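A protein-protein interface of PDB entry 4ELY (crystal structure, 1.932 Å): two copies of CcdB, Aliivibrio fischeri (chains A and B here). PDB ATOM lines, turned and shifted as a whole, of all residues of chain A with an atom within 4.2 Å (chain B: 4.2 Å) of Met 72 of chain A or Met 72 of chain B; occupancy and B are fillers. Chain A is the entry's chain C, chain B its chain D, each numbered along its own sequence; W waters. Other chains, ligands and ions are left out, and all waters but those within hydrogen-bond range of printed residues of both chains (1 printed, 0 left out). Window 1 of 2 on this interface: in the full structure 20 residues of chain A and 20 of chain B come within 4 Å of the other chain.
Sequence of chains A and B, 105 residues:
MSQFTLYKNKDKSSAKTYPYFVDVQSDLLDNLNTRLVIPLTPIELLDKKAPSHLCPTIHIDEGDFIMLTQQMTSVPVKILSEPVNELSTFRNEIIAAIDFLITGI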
ATOM      1  N   VAL A  24       1.385  -0.150  29.579  1.00  0.00           N
ATOM      2  CA  VAL A  24       1.807   0.203  30.941  1.00  0.00           C
ATOM      3  C   VAL A  24       0.643   0.561  31.852  1.00  0.00           C
ATOM      4  O   VAL A  24       0.834   1.029  32.973  1.00  0.00           O
ATOM      5  CB  VAL A  24       2.876   1.326  30.977  1.00  0.00           C
ATOM      6  CG1 VAL A  24       4.124   0.875  30.220  1.00  0.00           C
ATOM      7  CG2 VAL A  24       2.313   2.644  30.397  1.00  0.00           C
ATOM      8  N   LEU A  36      -2.734   3.046  27.736  1.00  0.00           N
ATOM      9  CA  LEU A  36      -1.509   3.827  27.740  1.00  0.00           C
ATOM     10  C   LEU A  36      -0.367   2.892  27.373  1.00  0.00           C
ATOM     11  O   LEU A  36      -0.159   1.854  28.026  1.00  0.00           O
ATOM     12  CB  LEU A  36      -1.270   4.415  29.127  1.00  0.00           C
ATOM     13  CG  LEU A  36      -0.179   5.475  29.251  1.00  0.00           C
ATOM     14  CD1 LEU A  36      -0.582   6.716  28.471  1.00  0.00           C
ATOM     15  CD2 LEU A  36       0.051   5.824  30.724  1.00  0.00           C
ATOM     16  N   VAL A  37       0.368   3.238  26.318  1.00  0.00           N
ATOM     17  CA  VAL A  37       1.485   2.404  25.886  1.00  0.00           C
ATOM     18  C   VAL A  37       2.766   3.203  25.670  1.00  0.00           C
ATOM     19  O   VAL A  37       2.729   4.427  25.476  1.00  0.00           O
ATOM     20  CB  VAL A  37       1.143   1.628  24.587  1.00  0.00           C
ATOM     21  CG1 VAL A  37      -0.129   0.816  24.774  1.00  0.00           C
ATOM     22  CG2 VAL A  37       0.983   2.599  23.418  1.00  0.00           C
ATOM     23  N   ILE A  38       3.896   2.500  25.712  1.00  0.00           N
ATOM     24  CA  ILE A  38       5.196   3.106  25.443  1.00  0.00           C
ATOM     25  C   ILE A  38       5.861   2.374  24.275  1.00  0.00           C
ATOM     26  O   ILE A  38       6.041   1.145  24.314  1.00  0.00           O
ATOM     27  CB  ILE A  38       6.131   3.034  26.680  1.00  0.00           C
ATOM     28  CG1 ILE A  38       5.580   3.850  27.856  1.00  0.00           C
ATOM     29  CG2 ILE A  38       7.521   3.553  26.339  1.00  0.00           C
ATOM     30  CD1 ILE A  38       6.408   3.677  29.138  1.00  0.00           C
ATOM     31  N   LEU A  68      10.963   4.359  24.738  1.00  0.00           N
ATOM     32  CA  LEU A  68      10.828   5.803  24.597  1.00  0.00           C
ATOM     33  C   LEU A  68       9.691   6.288  25.481  1.00  0.00           C
ATOM     34  O   LEU A  68       8.601   6.578  24.995  1.00  0.00           O
ATOM     35  CB  LEU A  68      10.547   6.163  23.136  1.00  0.00           C
ATOM     36  CG  LEU A  68      11.673   5.749  22.196  1.00  0.00           C
ATOM     37  CD1 LEU A  68      11.317   6.050  20.747  1.00  0.00           C
ATOM     38  CD2 LEU A  68      12.944   6.469  22.586  1.00  0.00           C
ATOM     39  N   THR A  69       9.963   6.355  26.781  1.00  0.00           N
ATOM     40  CA  THR A  69       8.975   6.726  27.793  1.00  0.00           C
ATOM     41  C   THR A  69       8.328   8.080  27.497  1.00  0.00           C
ATOM     42  O   THR A  69       7.122   8.262  27.686  1.00  0.00           O
ATOM     43  CB  THR A  69       9.654   6.787  29.172  1.00  0.00           C
ATOM     44  OG1 THR A  69      10.394   5.572  29.396  1.00  0.00           O
ATOM     45  CG2 THR A  69       8.629   6.983  30.288  1.00  0.00           C
ATOM     46  N   GLN A  70       9.123   9.028  27.017  1.00  0.00           N
ATOM     47  CA  GLN A  70       8.594  10.355  26.726  1.00  0.00           C
ATOM     48  C   GLN A  70       7.611  10.333  25.561  1.00  0.00           C
ATOM     49  O   GLN A  70       6.809  11.249  25.425  1.00  0.00           O
ATOM     50  CB  GLN A  70       9.724  11.353  26.436  1.00  0.00           C
ATOM     51  CG  GLN A  70      10.404  11.175  25.073  1.00  0.00           C
ATOM     52  CD  GLN A  70      11.550  10.183  25.110  1.00  0.00           C
ATOM     53  OE1 GLN A  70      11.529   9.216  25.871  1.00  0.00           O
ATOM     54  NE2 GLN A  70      12.568  10.427  24.292  1.00  0.00           N
ATOM     55  N   GLN A  71       7.664   9.299  24.723  1.00  0.00           N
ATOM     56  CA  GLN A  71       6.740   9.226  23.594  1.00  0.00           C
ATOM     57  C   GLN A  71       5.540   8.358  23.943  1.00  0.00           C
ATOM     58  O   GLN A  71       4.836   7.850  23.067  1.00  0.00           O
ATOM     59  CB  GLN A  71       7.454   8.729  22.336  1.00  0.00           C
ATOM     60  CG  GLN A  71       8.531   9.696  21.864  1.00  0.00           C
ATOM     61  CD  GLN A  71       9.182   9.280  20.560  1.00  0.00           C
ATOM     62  OE1 GLN A  71       8.661   8.433  19.830  1.00  0.00           O
ATOM     63  NE2 GLN A  71      10.333   9.877  20.260  1.00  0.00           N
ATOM     64  N   MET A  72       5.314   8.194  25.240  1.00  0.00           N
ATOM     65  CA  MET A  72       4.165   7.435  25.716  1.00  0.00           C
ATOM     66  C   MET A  72       2.861   8.018  25.172  1.00  0.00           C
ATOM     67  O   MET A  72       2.705   9.247  25.027  1.00  0.00           O
ATOM     68  CB  MET A  72       4.152   7.391  27.245  1.00  0.00           C
ATOM     69  CG  MET A  72       2.811   7.617  27.861  1.00  0.00           C
ATOM     70  SD  MET A  72       2.947   7.915  29.625  1.00  0.00           S
ATOM     71  CE  MET A  72       3.460   6.294  30.111  1.00  0.00           C
ATOM     72  N   THR A  73       1.930   7.134  24.833  1.00  0.00           N
ATOM     73  CA  THR A  73       0.697   7.581  24.204  1.00  0.00           C
ATOM     74  C   THR A  73      -0.481   6.655  24.479  1.00  0.00           C
ATOM     75  O   THR A  73      -0.313   5.479  24.809  1.00  0.00           O
ATOM     76  CB  THR A  73       0.874   7.786  22.679  1.00  0.00           C
ATOM     77  OG1 THR A  73      -0.282   8.443  22.139  1.00  0.00           O
ATOM     78  CG2 THR A  73       1.084   6.444  21.968  1.00  0.00           C
ATOM     79  N   SER A  74      -1.677   7.212  24.336  1.00  0.00           N
ATOM     80  CA  SER A  74      -2.913   6.476  24.518  1.00  0.00           C
ATOM     81  C   SER A  74      -3.371   5.937  23.162  1.00  0.00           C
ATOM     82  O   SER A  74      -3.412   6.673  22.178  1.00  0.00           O
ATOM     83  CB  SER A  74      -3.973   7.426  25.085  1.00  0.00           C
ATOM     84  OG  SER A  74      -5.196   6.757  25.306  1.00  0.00           O
ATOM     85  N   ILE A  98       8.696   6.512  34.170  1.00  0.00           N
ATOM     86  CA  ILE A  98       7.479   7.323  34.165  1.00  0.00           C
ATOM     87  C   ILE A  98       7.509   8.328  35.320  1.00  0.00           C
ATOM     88  O   ILE A  98       7.105   9.487  35.160  1.00  0.00           O
ATOM     89  CB  ILE A  98       6.222   6.431  34.253  1.00  0.00           C
ATOM     90  CG1 ILE A  98       6.126   5.550  33.006  1.00  0.00           C
ATOM     91  CG2 ILE A  98       4.963   7.287  34.429  1.00  0.00           C
ATOM     92  CD1 ILE A  98       5.096   4.427  33.111  1.00  0.00           C
ATOM     93  N   VAL B  24       2.079  17.943  31.566  1.00  0.00           N
ATOM     94  CA  VAL B  24       2.302  17.280  32.856  1.00  0.00           C
ATOM     95  C   VAL B  24       3.728  16.780  32.990  1.00  0.00           C
ATOM     96  O   VAL B  24       4.052  16.025  33.904  1.00  0.00           O
ATOM     97  CB  VAL B  24       1.322  16.106  33.091  1.00  0.00           C
ATOM     98  CG1 VAL B  24      -0.117  16.642  33.127  1.00  0.00           C
ATOM     99  CG2 VAL B  24       1.497  15.035  32.005  1.00  0.00           C
ATOM    100  N   LEU B  36       4.722  15.555  27.381  1.00  0.00           N
ATOM    101  CA  LEU B  36       3.588  14.715  27.729  1.00  0.00           C
ATOM    102  C   LEU B  36       2.452  15.621  28.180  1.00  0.00           C
ATOM    103  O   LEU B  36       2.615  16.418  29.116  1.00  0.00           O
ATOM    104  CB  LEU B  36       3.972  13.772  28.871  1.00  0.00           C
ATOM    105  CG  LEU B  36       2.930  12.703  29.205  1.00  0.00           C
ATOM    106  CD1 LEU B  36       2.674  11.794  28.005  1.00  0.00           C
ATOM    107  CD2 LEU B  36       3.391  11.870  30.377  1.00  0.00           C
ATOM    108  N   VAL B  37       1.306  15.529  27.514  1.00  0.00           N
ATOM    109  CA  VAL B  37       0.183  16.397  27.873  1.00  0.00           C
ATOM    110  C   VAL B  37      -1.101  15.606  28.083  1.00  0.00           C
ATOM    111  O   VAL B  37      -1.226  14.474  27.618  1.00  0.00           O
ATOM    112  CB  VAL B  37      -0.085  17.517  26.824  1.00  0.00           C
ATOM    113  CG1 VAL B  37       1.168  18.356  26.563  1.00  0.00           C
ATOM    114  CG2 VAL B  37      -0.635  16.929  25.524  1.00  0.00           C
ATOM    115  N   ILE B  38      -2.046  16.211  28.794  1.00  0.00           N
ATOM    116  CA  ILE B  38      -3.360  15.616  28.992  1.00  0.00           C
ATOM    117  C   ILE B  38      -4.439  16.553  28.451  1.00  0.00           C
ATOM    118  O   ILE B  38      -4.495  17.726  28.838  1.00  0.00           O
ATOM    119  CB  ILE B  38      -3.650  15.378  30.483  1.00  0.00           C
ATOM    120  CG1 ILE B  38      -2.643  14.406  31.097  1.00  0.00           C
ATOM    121  CG2 ILE B  38      -5.050  14.825  30.662  1.00  0.00           C
ATOM    122  CD1 ILE B  38      -2.886  14.168  32.575  1.00  0.00           C
ATOM    123  N   LEU B  68      -8.916  14.286  30.813  1.00  0.00           N
ATOM    124  CA  LEU B  68      -8.954  12.908  30.324  1.00  0.00           C
ATOM    125  C   LEU B  68      -7.578  12.265  30.438  1.00  0.00           C
ATOM    126  O   LEU B  68      -6.884  12.096  29.431  1.00  0.00           O
ATOM    127  CB  LEU B  68      -9.416  12.875  28.869  1.00  0.00           C
ATOM    128  CG  LEU B  68     -10.799  13.467  28.615  1.00  0.00           C
ATOM    129  CD1 LEU B  68     -11.076  13.519  27.132  1.00  0.00           C
ATOM    130  CD2 LEU B  68     -11.860  12.643  29.324  1.00  0.00           C
ATOM    131  N   THR B  69      -7.185  11.906  31.656  1.00  0.00           N
ATOM    132  CA  THR B  69      -5.823  11.424  31.895  1.00  0.00           C
ATOM    133  C   THR B  69      -5.495  10.160  31.100  1.00  0.00           C
ATOM    134  O   THR B  69      -4.350   9.949  30.737  1.00  0.00           O
ATOM    135  CB  THR B  69      -5.516  11.232  33.393  1.00  0.00           C
ATOM    136  OG1 THR B  69      -5.990   9.958  33.829  1.00  0.00           O
ATOM    137  CG2 THR B  69      -6.180  12.326  34.197  1.00  0.00           C
ATOM    138  N   GLN B  70      -6.503   9.350  30.794  1.00  0.00           N
ATOM    139  CA  GLN B  70      -6.261   8.128  30.027  1.00  0.00           C
ATOM    140  C   GLN B  70      -5.993   8.435  28.558  1.00  0.00           C
ATOM    141  O   GLN B  70      -5.497   7.583  27.828  1.00  0.00           O
ATOM    142  CB  GLN B  70      -7.424   7.135  30.154  1.00  0.00           C
ATOM    143  CG  GLN B  70      -8.670   7.487  29.347  1.00  0.00           C
ATOM    144  CD  GLN B  70      -9.632   8.364  30.127  1.00  0.00           C
ATOM    145  OE1 GLN B  70      -9.218   9.227  30.904  1.00  0.00           O
ATOM    146  NE2 GLN B  70     -10.926   8.130  29.941  1.00  0.00           N
ATOM    147  N   GLN B  71      -6.311   9.652  28.124  1.00  0.00           N
ATOM    148  CA  GLN B  71      -6.021  10.058  26.752  1.00  0.00           C
ATOM    149  C   GLN B  71      -4.746  10.889  26.699  1.00  0.00           C
ATOM    150  O   GLN B  71      -4.510  11.650  25.756  1.00  0.00           O
ATOM    151  CB  GLN B  71      -7.209  10.798  26.138  1.00  0.00           C
ATOM    152  CG  GLN B  71      -8.425   9.899  25.986  1.00  0.00           C
ATOM    153  CD  GLN B  71      -9.562  10.552  25.240  1.00  0.00           C
ATOM    154  OE1 GLN B  71      -9.353  11.443  24.414  1.00  0.00           O
ATOM    155  NE2 GLN B  71     -10.781  10.111  25.526  1.00  0.00           N
ATOM    156  N   MET B  72      -3.933  10.734  27.734  1.00  0.00           N
ATOM    157  CA  MET B  72      -2.639  11.396  27.839  1.00  0.00           C
ATOM    158  C   MET B  72      -1.801  10.969  26.641  1.00  0.00           C
ATOM    159  O   MET B  72      -1.862   9.814  26.202  1.00  0.00           O
ATOM    160  CB  MET B  72      -1.954  10.970  29.143  1.00  0.00           C
ATOM    161  CG  MET B  72      -0.677  11.712  29.528  1.00  0.00           C
ATOM    162  SD  MET B  72      -0.113  11.274  31.224  1.00  0.00           S
ATOM    163  CE  MET B  72      -0.065   9.487  31.102  1.00  0.00           C
ATOM    164  N   THR B  73      -1.038  11.902  26.091  1.00  0.00           N
ATOM    165  CA  THR B  73      -0.232  11.595  24.923  1.00  0.00           C
ATOM    166  C   THR B  73       0.935  12.564  24.834  1.00  0.00           C
ATOM    167  O   THR B  73       0.953  13.600  25.497  1.00  0.00           O
ATOM    168  CB  THR B  73      -1.074  11.640  23.619  1.00  0.00           C
ATOM    169  OG1 THR B  73      -0.284  11.179  22.513  1.00  0.00           O
ATOM    170  CG2 THR B  73      -1.562  13.056  23.342  1.00  0.00           C
ATOM    171  N   SER B  74       1.914  12.221  24.014  1.00  0.00           N
ATOM    172  CA  SER B  74       3.055  13.096  23.838  1.00  0.00           C
ATOM    173  C   SER B  74       2.906  13.867  22.535  1.00  0.00           C
ATOM    174  O   SER B  74       2.508  13.318  21.505  1.00  0.00           O
ATOM    175  CB  SER B  74       4.359  12.302  23.853  1.00  0.00           C
ATOM    176  OG  SER B  74       4.419  11.412  22.759  1.00  0.00           O
ATOM    177  N   ILE B  98      -2.758  10.070  37.361  1.00  0.00           N
ATOM    178  CA  ILE B  98      -1.760   9.356  36.583  1.00  0.00           C
ATOM    179  C   ILE B  98      -1.323   8.106  37.344  1.00  0.00           C
ATOM    180  O   ILE B  98      -1.195   7.038  36.747  1.00  0.00           O
ATOM    181  CB  ILE B  98      -0.537  10.246  36.240  1.00  0.00           C
ATOM    182  CG1 ILE B  98      -0.954  11.365  35.274  1.00  0.00           C
ATOM    183  CG2 ILE B  98       0.552   9.412  35.587  1.00  0.00           C
ATOM    184  CD1 ILE B  98       0.082  12.480  35.119  1.00  0.00           C
HETATM  185  O   HOH W   1       1.884  10.116  20.547  1.00  0.00           O
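Of the printed residues of chain B, Gln 70 of chain A touches Ser 74 (3.1 Å). Printed residues of chain B within 4 Å of Met 72 of chain A: Leu 36 (3.9 Å), Met 72 (3.7 Å), Thr 73 (3.8 Å) and Ser 74 (3.2 Å). Val 37 of chain B touches none of the printed residues of chain A. Printed residues of chain A within 4 Å of Gln 70 of chain B: Ser 74. Of the printed residues of chain A, Gln 71 of chain B touches Ser 74 (3.7 Å). Met 72 of chain B touches just these residues of chain A: Leu 36 (3.7 Å), Met 72 (3.7 Å), Thr 73 (3.9 Å) and Ser 74 (3.2 Å). Printed residues of chain A within 4 Å of Ser 74 of chain B: Gln 70, Gln 71 and Met 72. The nearest printed residue of chain B that does not touch Met 72 of chain A is Ile 98 of chain B (6.6 Å). The nearest printed residue of chain A that does not touch Met 72 of chain B is Ile 98 of chain A (6.4 Å).
Among the printed residues, merely in contact across the chains: Gln 70 of chain A with Ser 74 of chain B, Gln 71 of chain A with Ser 74 of chain B, Leu 36 of chain A with Met 72 of chain B, Ser 74 of chain A with Gln 71 of chain B, Met 72 of chain A with Met 72 of chain B, Met 72 of chain A with Thr 73 of chain B, Thr 73 of chain A with Met 72 of chain B and Met 72 of chain A with Leu 36 of chain B.
O of Leu 36 of chain A sits at hydrogen-bond distance from N of Val 24 of chain A, 3.0 Å away. The backbone NH (N) of Val 37 of chain B lies within hydrogen-bond range of the backbone carbonyl oxygen (O) of Thr 73 of chain B. N of Val 37 of chain A is in hydrogen-bond range of O of Thr 73 of chain A (2.8 Å). N of Val 24 of chain B sits at hydrogen-bond distance from O of Leu 36 of chain B (2.9 Å).
Water W1 lies within hydrogen-bond range of the side-chain hydroxyl of Thr 73 of chain B (3.1 Å), the side-chain hydroxyl of Thr 73 of chain A (3.2 Å) and the backbone carbonyl oxygen of Ser 74 of chain B (3.4 Å).
Printed residues of chain B that touch a printed residue of chain A: Leu 36, Gln 70, Gln 71, Met 72, Thr 73 and Ser 74. Hydrophobic or aromatic side chains of chain B that line the printed part of chain A: Leu 36 and Met 72. Hydrophobic or aromatic side chains of chain A that line the printed part of chain B: Leu 36 and Met 72. Among the printed residues, 12 pairs touch across the chains. Among the printed residues, no Asp or Glu carboxylate lies within 4 Å of a Lys or Arg side-chain nitrogen of the other chain.
The side-chain hydroxyl of Thr 73 of chain A sits at hydrogen-bond distance from the side-chain hydroxyl of Thr 73 of chain B, at 2.8 Å. N of Ser 74 of chain A lies within hydrogen-bond range of O of Met 72 of chain B, at 3.2 Å. The backbone carbonyl oxygen (O) of Met 72 of chain A is in hydrogen-bond range of the backbone NH (N) of Ser 74 of chain B (3.2 Å). The side-chain hydroxyl (OG) of Ser 74 of chain A is in hydrogen-bond range of the backbone carbonyl oxygen (O) of Gln 70 of chain B.
Gln 71 of chain A touches Ser 74 of chain B, and with the chains exchanged Ser 74 of chain A touches Gln 71 of chain B. Met 72 of chain B touches its own counterpart, Met 72 of chain A. Met 72 of chain A touches Thr 73 of chain B, and with the chains exchanged Thr 73 of chain A touches Met 72 of chain B. Met 72 of chain A touches Ser 74 of chain B, and with the chains exchanged Ser 74 of chain A touches Met 72 of chain B. Positions printed for both chains: 24, 36, 37, 38, 68, 69, 70, 71, 72, 73, 74 and 98.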
